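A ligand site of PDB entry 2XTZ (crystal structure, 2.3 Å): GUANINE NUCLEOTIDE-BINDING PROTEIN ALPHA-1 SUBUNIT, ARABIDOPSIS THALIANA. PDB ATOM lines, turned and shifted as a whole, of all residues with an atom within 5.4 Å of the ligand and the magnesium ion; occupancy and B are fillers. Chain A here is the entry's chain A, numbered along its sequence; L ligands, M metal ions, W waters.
O3 of the ligand sits close to N of Thr 164, 3.1 Å away.
The backbone NH (N) of Ser 23 is in hydrogen-bond range of an oxygen (O6) of the ligand.
The backbone NH (N) of Thr 24 lies within hydrogen-bond range of an oxygen (O6) of the ligand, at 2.9 Å.
An oxygen (O6) of the ligand is in hydrogen-bond range of the side-chain hydroxyl of Thr 24, 2.5 Å away.
The backbone carbonyl oxygen of Tyr 159 lies within hydrogen-bond range of an oxygen (O11) of the ligand, 2.7 Å away.
O of Leu 158 is in hydrogen-bond range of O12 of the ligand (2.7 Å).
N of Gly 192 sits at hydrogen-bond distance from O2 of the ligand, 2.7 Å away.
OD2 of Asp 261 lies within hydrogen-bond range of N4 of the ligand (2.7 Å).
N of Lys 22 lies within hydrogen-bond range of O4 of the ligand (3.0 Å).
An oxygen (O4) of the ligand is in salt-bridge range of the side-chain amino group (NZ) of Lys 22, at 2.9 Å.
The backbone NH (N) of Glu 19 sits at hydrogen-bond distance from an oxygen (O1) of the ligand, 2.9 Å away.
N of Ala 326 sits at hydrogen-bond distance from O13 of the ligand (3.0 Å).
O8 of the ligand is in hydrogen-bond range of N of Gly 21 (3.1 Å).
ND2 of Asn 258 sits at hydrogen-bond distance from N2 of the ligand (3.1 Å).
The backbone NH of Ser 20 is in hydrogen-bond range of an oxygen (O4) of the ligand.
OG of Ser 20 lies within hydrogen-bond range of O4 of the ligand (3.4 Å).
An oxygen (O13) of the ligand lies within hydrogen-bond range of the backbone NH of Lys 259 (3.2 Å).
The side-chain amino group (NZ) of Lys 259 lies within hydrogen-bond range of an oxygen (O10) of the ligand (3.1 Å).
SD of CSS 134 is in hydrogen-bond range of an oxygen (O11) of the ligand, at 3.8 Å.
N of Gly 18 is in hydrogen-bond range of O of Gly 192.
The backbone NH (N) of Asp 261 is in hydrogen-bond range of the side-chain hydroxyl (OG1) of Thr 325, 3.2 Å away.
The backbone carbonyl oxygen (O) of Gly 16 is in hydrogen-bond range of the side-chain amino group (NZ) of Lys 22.
The backbone carbonyl oxygen (O) of Glu 19 is in hydrogen-bond range of the side-chain amino group (NZ) of Lys 259, at 2.7 Å.
NH1 of Arg 161 is in salt-bridge range of OE2 of Glu 19 (3.8 Å).
The side-chain amide oxygen of Asn 258 lies within hydrogen-bond range of the backbone NH of Ala 326 (3.0 Å).
The side-chain hydroxyl (OG) of Ser 20 is in hydrogen-bond range of the backbone carbonyl oxygen (O) of Ala 17 (2.9 Å).
The side-chain amide oxygen (OE1) of Gln 193 sits at hydrogen-bond distance from the guanidinium group (NH1) of Arg 163, 2.8 Å away.
O of Ala 17 touches O4 of the ligand (3.9 Å).
Gly 18 touches the ligand (CA to O2, 3.6 Å).
Arg 161 touches the ligand.
Arg 163 touches the ligand.
C of Gly 191 touches O2 of the ligand, at 3.7 Å.
CD1 of Ile 262 touches N4 of the ligand, at 3.3 Å.
Thr 325 touches the ligand.
CD2 of Leu 327 touches O12 of the ligand (3.6 Å).
Hydrophobic or aromatic side chains that line the ligand: Ile 262, Ala 326 and Leu 327.
The nearest printed residue that does not touch the ligand is Gln 193 (4.02 Å).
Residues that only touch the magnesium ion: Asp 189 (3.9 Å).
Three residues have an atom within 4 Å of the magnesium ion: Ser 23, Thr 164 and Asp 189.
The nearest printed residue that does not touch the magnesium ion is Val 162 (4.5 Å).
The magnesium ion is bound by OG1 of Thr 164 (2.1 Å), water W3 (2.1 Å), OG of Ser 23 (2.1 Å), O3 of the ligand (2.2 Å), O5 of the ligand (2.2 Å) and water W4 (2.3 Å).
The magnesium ion has six donor atoms within binding distance.
Water W3 lies within hydrogen-bond range of O of Val 190 (2.5 Å) and OD1 of Asp 189 (2.8 Å).
Water W4 bridges O of Val 162 (2.6 Å) and O7 of the ligand (2.7 Å).
Water W5 lies within hydrogen-bond range of O7 of the ligand (2.9 Å), N of Val 162 (2.9 Å) and O of Ala 160 (3.0 Å).
Water W7 lies within hydrogen-bond range of S1 of the ligand (3.1 Å), O of Thr 164 (3.1 Å) and N of Gln 193 (3.4 Å).
Water W1 lies within hydrogen-bond range of an oxygen (O11) of the ligand (3.2 Å) and N of CSS 134 (3.2 Å).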
ATOM      1  N   GLY A  16      -7.267  36.539  26.465  1.00  0.00           N
ATOM      2  CA  GLY A  16      -7.162  35.274  27.146  1.00  0.00           C
ATOM      3  C   GLY A  16      -6.112  34.404  26.462  1.00  0.00           C
ATOM      4  O   GLY A  16      -5.756  34.635  25.316  1.00  0.00           O
ATOM      5  N   ALA A  17      -5.645  33.392  27.186  1.00  0.00           N
ATOM      6  CA  ALA A  17      -4.621  32.471  26.706  1.00  0.00           C
ATOM      7  C   ALA A  17      -5.062  31.684  25.457  1.00  0.00           C
ATOM      8  O   ALA A  17      -6.242  31.692  25.081  1.00  0.00           O
ATOM      9  CB  ALA A  17      -4.288  31.526  27.803  1.00  0.00           C
ATOM     10  N   GLY A  18      -4.111  31.010  24.810  1.00  0.00           N
ATOM     11  CA  GLY A  18      -4.462  30.110  23.691  1.00  0.00           C
ATOM     12  C   GLY A  18      -5.535  29.110  24.100  1.00  0.00           C
ATOM     13  O   GLY A  18      -5.484  28.538  25.213  1.00  0.00           O
ATOM     14  N   GLU A  19      -6.521  28.925  23.222  1.00  0.00           N
ATOM     15  CA  GLU A  19      -7.548  27.882  23.350  1.00  0.00           C
ATOM     16  C   GLU A  19      -8.588  28.166  24.428  1.00  0.00           C
ATOM     17  O   GLU A  19      -9.298  27.253  24.864  1.00  0.00           O
ATOM     18  CB  GLU A  19      -6.930  26.482  23.563  1.00  0.00           C
ATOM     19  CG  GLU A  19      -6.212  25.889  22.326  1.00  0.00           C
ATOM     20  CD  GLU A  19      -5.355  24.664  22.659  1.00  0.00           C
ATOM     21  OE1 GLU A  19      -4.210  24.590  22.201  1.00  0.00           O
ATOM     22  OE2 GLU A  19      -5.806  23.756  23.387  1.00  0.00           O
ATOM     23  N   SER A  20      -8.702  29.412  24.848  1.00  0.00           N
ATOM     24  CA  SER A  20      -9.582  29.703  25.973  1.00  0.00           C
ATOM     25  C   SER A  20     -11.029  29.880  25.560  1.00  0.00           C
ATOM     26  O   SER A  20     -11.886  29.840  26.417  1.00  0.00           O
ATOM     27  CB  SER A  20      -9.097  30.916  26.750  1.00  0.00           C
ATOM     28  OG  SER A  20      -9.004  32.015  25.873  1.00  0.00           O
ATOM     29  N   GLY A  21     -11.294  30.056  24.269  1.00  0.00           N
ATOM     30  CA  GLY A  21     -12.668  30.170  23.781  1.00  0.00           C
ATOM     31  C   GLY A  21     -13.023  31.463  23.075  1.00  0.00           C
ATOM     32  O   GLY A  21     -14.187  31.666  22.728  1.00  0.00           O
ATOM     33  N   LYS A  22     -12.035  32.333  22.851  1.00  0.00           N
ATOM     34  CA  LYS A  22     -12.270  33.660  22.255  1.00  0.00           C
ATOM     35  C   LYS A  22     -12.956  33.599  20.883  1.00  0.00           C
ATOM     36  O   LYS A  22     -13.986  34.236  20.674  1.00  0.00           O
ATOM     37  CB  LYS A  22     -10.947  34.453  22.167  1.00  0.00           C
ATOM     38  CG  LYS A  22     -10.313  34.762  23.544  1.00  0.00           C
ATOM     39  CD  LYS A  22      -8.971  35.463  23.434  1.00  0.00           C
ATOM     40  CE  LYS A  22      -7.951  34.702  22.565  1.00  0.00           C
ATOM     41  NZ  LYS A  22      -7.335  33.520  23.230  1.00  0.00           N
ATOM     42  N   SER A  23     -12.396  32.835  19.964  1.00  0.00           N
ATOM     43  CA  SER A  23     -12.983  32.748  18.626  1.00  0.00           C
ATOM     44  C   SER A  23     -14.376  32.125  18.668  1.00  0.00           C
ATOM     45  O   SER A  23     -15.226  32.459  17.863  1.00  0.00           O
ATOM     46  CB  SER A  23     -12.086  31.964  17.684  1.00  0.00           C
ATOM     47  OG  SER A  23     -10.852  32.639  17.499  1.00  0.00           O
ATOM     48  N   THR A  24     -14.589  31.237  19.641  1.00  0.00           N
ATOM     49  CA  THR A  24     -15.836  30.524  19.769  1.00  0.00           C
ATOM     50  C   THR A  24     -16.898  31.514  20.199  1.00  0.00           C
ATOM     51  O   THR A  24     -18.001  31.546  19.610  1.00  0.00           O
ATOM     52  CB  THR A  24     -15.673  29.337  20.745  1.00  0.00           C
ATOM     53  OG1 THR A  24     -14.617  28.508  20.267  1.00  0.00           O
ATOM     54  CG2 THR A  24     -16.922  28.501  20.807  1.00  0.00           C
ATOM     55  N   ILE A  25     -16.554  32.350  21.178  1.00  0.00           N
ATOM     56  CA  ILE A  25     -17.410  33.455  21.599  1.00  0.00           C
ATOM     57  C   ILE A  25     -17.673  34.410  20.420  1.00  0.00           C
ATOM     58  O   ILE A  25     -18.826  34.810  20.188  1.00  0.00           O
ATOM     59  CB  ILE A  25     -16.828  34.229  22.813  1.00  0.00           C
ATOM     60  CG1 ILE A  25     -16.849  33.359  24.093  1.00  0.00           C
ATOM     61  CG2 ILE A  25     -17.576  35.546  23.058  1.00  0.00           C
ATOM     62  CD1 ILE A  25     -18.235  33.089  24.700  1.00  0.00           C
ATOM     63  N   CSS A 134     -12.392  18.064  22.251  1.00  0.00           N
ATOM     64  CA  CSS A 134     -13.414  17.665  21.262  1.00  0.00           C
ATOM     65  CB  CSS A 134     -13.399  18.688  20.123  1.00  0.00           C
ATOM     66  SG  CSS A 134     -11.923  18.461  19.178  1.00  0.00           S
ATOM     67  SD  CSS A 134     -11.473  20.173  18.178  1.00  0.00           S
ATOM     68  C   CSS A 134     -13.199  16.257  20.712  1.00  0.00           C
ATOM     69  O   CSS A 134     -13.959  15.809  19.858  1.00  0.00           O
ATOM     70  N   LEU A 158     -18.565  25.396  15.551  1.00  0.00           N
ATOM     71  CA  LEU A 158     -18.178  26.001  16.808  1.00  0.00           C
ATOM     72  C   LEU A 158     -17.058  25.183  17.441  1.00  0.00           C
ATOM     73  O   LEU A 158     -16.135  25.746  18.041  1.00  0.00           O
ATOM     74  CB  LEU A 158     -19.382  26.125  17.751  1.00  0.00           C
ATOM     75  CG  LEU A 158     -20.340  27.280  17.476  1.00  0.00           C
ATOM     76  CD1 LEU A 158     -21.676  26.991  18.119  1.00  0.00           C
ATOM     77  CD2 LEU A 158     -19.802  28.607  17.987  1.00  0.00           C
ATOM     78  N   TYR A 159     -17.168  23.861  17.300  1.00  0.00           N
ATOM     79  CA  TYR A 159     -16.075  22.956  17.614  1.00  0.00           C
ATOM     80  C   TYR A 159     -14.826  23.227  16.772  1.00  0.00           C
ATOM     81  O   TYR A 159     -13.724  23.254  17.329  1.00  0.00           O
ATOM     82  CB  TYR A 159     -16.492  21.508  17.444  1.00  0.00           C
ATOM     83  CG  TYR A 159     -16.996  20.896  18.726  1.00  0.00           C
ATOM     84  CD1 TYR A 159     -16.104  20.592  19.756  1.00  0.00           C
ATOM     85  CD2 TYR A 159     -18.332  20.610  18.912  1.00  0.00           C
ATOM     86  CE1 TYR A 159     -16.531  20.022  20.947  1.00  0.00           C
ATOM     87  CE2 TYR A 159     -18.768  20.032  20.111  1.00  0.00           C
ATOM     88  CZ  TYR A 159     -17.858  19.747  21.117  1.00  0.00           C
ATOM     89  OH  TYR A 159     -18.249  19.178  22.298  1.00  0.00           O
ATOM     90  N   ALA A 160     -14.997  23.430  15.461  1.00  0.00           N
ATOM     91  CA  ALA A 160     -13.879  23.591  14.534  1.00  0.00           C
ATOM     92  C   ALA A 160     -12.786  24.503  15.093  1.00  0.00           C
ATOM     93  O   ALA A 160     -13.039  25.642  15.514  1.00  0.00           O
ATOM     94  CB  ALA A 160     -14.367  24.109  13.173  1.00  0.00           C
ATOM     95  N   ARG A 161     -11.563  24.002  15.077  1.00  0.00           N
ATOM     96  CA  ARG A 161     -10.480  24.637  15.780  1.00  0.00           C
ATOM     97  C   ARG A 161      -9.345  25.104  14.880  1.00  0.00           C
ATOM     98  O   ARG A 161      -8.640  24.291  14.275  1.00  0.00           O
ATOM     99  CB  ARG A 161      -9.922  23.736  16.897  1.00  0.00           C
ATOM    100  CG  ARG A 161      -8.982  24.502  17.848  1.00  0.00           C
ATOM    101  CD  ARG A 161      -8.450  23.603  18.912  1.00  0.00           C
ATOM    102  NE  ARG A 161      -7.353  22.763  18.430  1.00  0.00           N
ATOM    103  CZ  ARG A 161      -6.716  21.862  19.165  1.00  0.00           C
ATOM    104  NH1 ARG A 161      -7.068  21.661  20.439  1.00  0.00           N
ATOM    105  NH2 ARG A 161      -5.719  21.161  18.637  1.00  0.00           N
ATOM    106  N   VAL A 162      -9.184  26.430  14.821  1.00  0.00           N
ATOM    107  CA  VAL A 162      -8.066  27.094  14.162  1.00  0.00           C
ATOM    108  C   VAL A 162      -7.404  28.002  15.203  1.00  0.00           C
ATOM    109  O   VAL A 162      -8.104  28.755  15.882  1.00  0.00           O
ATOM    110  CB  VAL A 162      -8.531  27.985  12.958  1.00  0.00           C
ATOM    111  CG1 VAL A 162      -7.316  28.616  12.246  1.00  0.00           C
ATOM    112  CG2 VAL A 162      -9.296  27.155  11.933  1.00  0.00           C
ATOM    113  N   ARG A 163      -6.089  27.945  15.329  1.00  0.00           N
ATOM    114  CA  ARG A 163      -5.381  28.965  16.134  1.00  0.00           C
ATOM    115  C   ARG A 163      -5.407  30.317  15.412  1.00  0.00           C
ATOM    116  O   ARG A 163      -5.013  30.413  14.260  1.00  0.00           O
ATOM    117  CB  ARG A 163      -3.941  28.562  16.380  1.00  0.00           C
ATOM    118  CG  ARG A 163      -3.789  27.316  17.228  1.00  0.00           C
ATOM    119  CD  ARG A 163      -2.351  27.079  17.449  1.00  0.00           C
ATOM    120  NE  ARG A 163      -1.625  26.709  16.218  1.00  0.00           N
ATOM    121  CZ  ARG A 163      -0.305  26.809  16.081  1.00  0.00           C
ATOM    122  NH1 ARG A 163       0.435  27.301  17.089  1.00  0.00           N
ATOM    123  NH2 ARG A 163       0.284  26.444  14.946  1.00  0.00           N
ATOM    124  N   THR A 164      -5.869  31.359  16.092  1.00  0.00           N
ATOM    125  CA  THR A 164      -6.017  32.669  15.449  1.00  0.00           C
ATOM    126  C   THR A 164      -4.669  33.345  15.319  1.00  0.00           C
ATOM    127  O   THR A 164      -3.918  33.420  16.282  1.00  0.00           O
ATOM    128  CB  THR A 164      -7.009  33.561  16.238  1.00  0.00           C
ATOM    129  OG1 THR A 164      -8.210  32.819  16.494  1.00  0.00           O
ATOM    130  CG2 THR A 164      -7.345  34.866  15.462  1.00  0.00           C
ATOM    131  N   ASP A 189     -11.222  40.119  17.869  1.00  0.00           N
ATOM    132  CA  ASP A 189     -10.693  38.801  18.185  1.00  0.00           C
ATOM    133  C   ASP A 189      -9.228  38.785  17.763  1.00  0.00           C
ATOM    134  O   ASP A 189      -8.879  39.299  16.699  1.00  0.00           O
ATOM    135  CB  ASP A 189     -11.448  37.700  17.424  1.00  0.00           C
ATOM    136  CG  ASP A 189     -11.080  36.276  17.901  1.00  0.00           C
ATOM    137  OD1 ASP A 189     -10.655  36.103  19.078  1.00  0.00           O
ATOM    138  OD2 ASP A 189     -11.249  35.328  17.087  1.00  0.00           O
ATOM    139  N   VAL A 190      -8.388  38.174  18.606  1.00  0.00           N
ATOM    140  CA  VAL A 190      -6.948  38.129  18.429  1.00  0.00           C
ATOM    141  C   VAL A 190      -6.456  36.780  19.010  1.00  0.00           C
ATOM    142  O   VAL A 190      -7.135  36.200  19.833  1.00  0.00           O
ATOM    143  CB  VAL A 190      -6.309  39.361  19.140  1.00  0.00           C
ATOM    144  CG1 VAL A 190      -6.590  39.328  20.646  1.00  0.00           C
ATOM    145  CG2 VAL A 190      -4.800  39.463  18.868  1.00  0.00           C
ATOM    146  N   GLY A 191      -5.313  36.276  18.555  1.00  0.00           N
ATOM    147  CA  GLY A 191      -4.727  35.043  19.105  1.00  0.00           C
ATOM    148  C   GLY A 191      -4.218  35.219  20.538  1.00  0.00           C
ATOM    149  O   GLY A 191      -3.774  36.315  20.921  1.00  0.00           O
ATOM    150  N   GLY A 192      -4.265  34.156  21.322  1.00  0.00           N
ATOM    151  CA  GLY A 192      -3.800  34.209  22.720  1.00  0.00           C
ATOM    152  C   GLY A 192      -2.583  33.352  23.042  1.00  0.00           C
ATOM    153  O   GLY A 192      -2.055  33.395  24.161  1.00  0.00           O
ATOM    154  N   GLN A 193      -2.137  32.555  22.089  1.00  0.00           N
ATOM    155  CA  GLN A 193      -0.863  31.879  22.276  1.00  0.00           C
ATOM    156  C   GLN A 193       0.210  32.930  22.407  1.00  0.00           C
ATOM    157  O   GLN A 193       0.087  34.031  21.847  1.00  0.00           O
ATOM    158  CB  GLN A 193      -0.572  30.875  21.160  1.00  0.00           C
ATOM    159  CG  GLN A 193      -1.447  29.633  21.283  1.00  0.00           C
ATOM    160  CD  GLN A 193      -1.076  28.519  20.341  1.00  0.00           C
ATOM    161  OE1 GLN A 193      -0.295  28.713  19.400  1.00  0.00           O
ATOM    162  NE2 GLN A 193      -1.630  27.341  20.586  1.00  0.00           N
ATOM    163  N   ASN A 258     -14.861  30.165  31.420  1.00  0.00           N
ATOM    164  CA  ASN A 258     -15.369  29.399  30.273  1.00  0.00           C
ATOM    165  C   ASN A 258     -15.070  27.897  30.338  1.00  0.00           C
ATOM    166  O   ASN A 258     -14.236  27.443  31.142  1.00  0.00           O
ATOM    167  CB  ASN A 258     -14.792  29.992  28.964  1.00  0.00           C
ATOM    168  CG  ASN A 258     -15.459  29.433  27.720  1.00  0.00           C
ATOM    169  OD1 ASN A 258     -16.700  29.401  27.627  1.00  0.00           O
ATOM    170  ND2 ASN A 258     -14.643  28.956  26.770  1.00  0.00           N
ATOM    171  N   LYS A 259     -15.761  27.124  29.484  1.00  0.00           N
ATOM    172  CA  LYS A 259     -15.675  25.643  29.469  1.00  0.00           C
ATOM    173  C   LYS A 259     -16.211  25.047  30.756  1.00  0.00           C
ATOM    174  O   LYS A 259     -15.706  24.045  31.271  1.00  0.00           O
ATOM    175  CB  LYS A 259     -14.256  25.170  29.157  1.00  0.00           C
ATOM    176  CG  LYS A 259     -13.710  25.753  27.855  1.00  0.00           C
ATOM    177  CD  LYS A 259     -12.493  25.016  27.253  1.00  0.00           C
ATOM    178  CE  LYS A 259     -11.932  25.837  26.101  1.00  0.00           C
ATOM    179  NZ  LYS A 259     -10.882  25.164  25.307  1.00  0.00           N
ATOM    180  N   PHE A 260     -17.271  25.650  31.279  1.00  0.00           N
ATOM    181  CA  PHE A 260     -17.917  25.085  32.459  1.00  0.00           C
ATOM    182  C   PHE A 260     -18.455  23.672  32.226  1.00  0.00           C
ATOM    183  O   PHE A 260     -18.404  22.828  33.144  1.00  0.00           O
ATOM    184  CB  PHE A 260     -19.027  26.015  32.941  1.00  0.00           C
ATOM    185  CG  PHE A 260     -19.711  25.489  34.156  1.00  0.00           C
ATOM    186  CD1 PHE A 260     -19.056  25.506  35.394  1.00  0.00           C
ATOM    187  CD2 PHE A 260     -20.988  24.959  34.063  1.00  0.00           C
ATOM    188  CE1 PHE A 260     -19.676  24.997  36.531  1.00  0.00           C
ATOM    189  CE2 PHE A 260     -21.622  24.454  35.201  1.00  0.00           C
ATOM    190  CZ  PHE A 260     -20.952  24.468  36.438  1.00  0.00           C
ATOM    191  N   ASP A 261     -19.002  23.410  31.038  1.00  0.00           N
ATOM    192  CA  ASP A 261     -19.430  22.047  30.644  1.00  0.00           C
ATOM    193  C   ASP A 261     -18.313  20.995  30.830  1.00  0.00           C
ATOM    194  O   ASP A 261     -18.568  19.904  31.303  1.00  0.00           O
ATOM    195  CB  ASP A 261     -19.945  22.017  29.200  1.00  0.00           C
ATOM    196  CG  ASP A 261     -18.849  22.352  28.156  1.00  0.00           C
ATOM    197  OD1 ASP A 261     -18.018  23.240  28.373  1.00  0.00           O
ATOM    198  OD2 ASP A 261     -18.801  21.719  27.097  1.00  0.00           O
ATOM    199  N   ILE A 262     -17.067  21.322  30.477  1.00  0.00           N
ATOM    200  CA  ILE A 262     -15.961  20.383  30.704  1.00  0.00           C
ATOM    201  C   ILE A 262     -15.554  20.296  32.189  1.00  0.00           C
ATOM    202  O   ILE A 262     -15.364  19.205  32.732  1.00  0.00           O
ATOM    203  CB  ILE A 262     -14.732  20.721  29.844  1.00  0.00           C
ATOM    204  CG1 ILE A 262     -15.106  20.682  28.356  1.00  0.00           C
ATOM    205  CG2 ILE A 262     -13.593  19.718  30.134  1.00  0.00           C
ATOM    206  CD1 ILE A 262     -13.979  21.236  27.435  1.00  0.00           C
ATOM    207  N   THR A 324     -19.391  30.464  31.753  1.00  0.00           N
ATOM    208  CA  THR A 324     -19.834  30.298  30.367  1.00  0.00           C
ATOM    209  C   THR A 324     -19.463  28.929  29.801  1.00  0.00           C
ATOM    210  O   THR A 324     -18.551  28.258  30.283  1.00  0.00           O
ATOM    211  CB  THR A 324     -19.328  31.423  29.432  1.00  0.00           C
ATOM    212  OG1 THR A 324     -17.908  31.318  29.285  1.00  0.00           O
ATOM    213  CG2 THR A 324     -19.673  32.813  29.985  1.00  0.00           C
ATOM    214  N   THR A 325     -20.238  28.519  28.812  1.00  0.00           N
ATOM    215  CA  THR A 325     -19.898  27.447  27.906  1.00  0.00           C
ATOM    216  C   THR A 325     -20.107  28.126  26.564  1.00  0.00           C
ATOM    217  O   THR A 325     -21.244  28.442  26.184  1.00  0.00           O
ATOM    218  CB  THR A 325     -20.807  26.246  28.095  1.00  0.00           C
ATOM    219  OG1 THR A 325     -20.499  25.634  29.346  1.00  0.00           O
ATOM    220  CG2 THR A 325     -20.604  25.196  26.962  1.00  0.00           C
ATOM    221  N   ALA A 326     -18.999  28.424  25.889  1.00  0.00           N
ATOM    222  CA  ALA A 326     -19.003  29.162  24.625  1.00  0.00           C
ATOM    223  C   ALA A 326     -19.760  28.452  23.484  1.00  0.00           C
ATOM    224  O   ALA A 326     -20.287  29.097  22.594  1.00  0.00           O
ATOM    225  CB  ALA A 326     -17.559  29.513  24.198  1.00  0.00           C
ATOM    226  N   LEU A 327     -19.818  27.129  23.536  1.00  0.00           N
ATOM    227  CA  LEU A 327     -20.600  26.353  22.573  1.00  0.00           C
ATOM    228  C   LEU A 327     -22.130  26.500  22.754  1.00  0.00           C
ATOM    229  O   LEU A 327     -22.898  26.147  21.860  1.00  0.00           O
ATOM    230  CB  LEU A 327     -20.242  24.849  22.638  1.00  0.00           C
ATOM    231  CG  LEU A 327     -18.808  24.327  22.660  1.00  0.00           C
ATOM    232  CD1 LEU A 327     -18.811  22.804  22.681  1.00  0.00           C
ATOM    233  CD2 LEU A 327     -18.064  24.827  21.447  1.00  0.00           C
HETATM  234  P1  LIG L   1      -6.505  30.981  20.202  1.00  0.00           P
HETATM  235  O1  LIG L   1      -7.701  30.128  20.886  1.00  0.00           O
HETATM  236  S1  LIG L   1      -5.192  29.843  19.828  1.00  0.00           S
HETATM  237  O2  LIG L   1      -6.030  32.108  21.139  1.00  0.00           O
HETATM  238  O3  LIG L   1      -7.013  31.674  18.936  1.00  0.00           O
HETATM  239  P2  LIG L   1      -9.213  30.650  21.247  1.00  0.00           P
HETATM  240  O4  LIG L   1      -9.162  31.429  22.509  1.00  0.00           O
HETATM  241  O5  LIG L   1      -9.806  31.419  20.135  1.00  0.00           O
HETATM  242  P3  LIG L   1     -11.073  28.723  20.490  1.00  0.00           P
HETATM  243  O6  LIG L   1     -12.302  29.560  20.447  1.00  0.00           O
HETATM  244  O7  LIG L   1     -10.495  28.522  19.148  1.00  0.00           O
HETATM  245  O8  LIG L   1     -10.049  29.333  21.544  1.00  0.00           O
HETATM  246  O9  LIG L   1     -11.412  27.330  21.192  1.00  0.00           O
HETATM  247  C1  LIG L   1     -10.500  26.277  21.205  1.00  0.00           C
HETATM  248  C2  LIG L   1     -11.296  24.976  21.212  1.00  0.00           C
HETATM  249  O10 LIG L   1     -12.045  24.880  22.411  1.00  0.00           O
HETATM  250  C3  LIG L   1     -12.297  24.905  20.055  1.00  0.00           C
HETATM  251  O11 LIG L   1     -12.280  23.588  19.566  1.00  0.00           O
HETATM  252  C4  LIG L   1     -13.652  25.217  20.692  1.00  0.00           C
HETATM  253  O12 LIG L   1     -14.738  24.603  20.061  1.00  0.00           O
HETATM  254  C5  LIG L   1     -13.429  24.704  22.105  1.00  0.00           C
HETATM  255  N1  LIG L   1     -14.223  25.416  23.118  1.00  0.00           N
HETATM  256  C6  LIG L   1     -14.242  26.775  23.346  1.00  0.00           C
HETATM  257  N2  LIG L   1     -15.072  27.008  24.376  1.00  0.00           N
HETATM  258  C7  LIG L   1     -15.565  25.831  24.825  1.00  0.00           C
HETATM  259  C8  LIG L   1     -16.450  25.495  25.851  1.00  0.00           C
HETATM  260  O13 LIG L   1     -16.936  26.354  26.560  1.00  0.00           O
HETATM  261  N3  LIG L   1     -16.778  24.175  26.091  1.00  0.00           N
HETATM  262  C9  LIG L   1     -16.229  23.186  25.303  1.00  0.00           C
HETATM  263  N4  LIG L   1     -16.551  21.923  25.531  1.00  0.00           N
HETATM  264  N5  LIG L   1     -15.359  23.522  24.288  1.00  0.00           N
HETATM  265  C10 LIG L   1     -15.038  24.817  24.039  1.00  0.00           C
HETATM  266 MG    MG M   1      -8.972  32.385  18.348  1.00  0.00          MG
HETATM  267  O   HOH W   1     -11.800  21.169  21.557  1.00  0.00           O
HETATM  268  O   HOH W   2      -7.527  27.518  19.388  1.00  0.00           O
HETATM  269  O   HOH W   3      -8.626  34.235  19.226  1.00  0.00           O
HETATM  270  O   HOH W   4      -9.366  30.335  17.438  1.00  0.00           O
HETATM  271  O   HOH W   5     -11.196  27.817  16.435  1.00  0.00           O
HETATM  272  O   HOH W   6     -13.947  21.269  23.234  1.00  0.00           O
HETATM  273  O   HOH W   7      -3.099  31.908  18.873  1.00  0.00           O
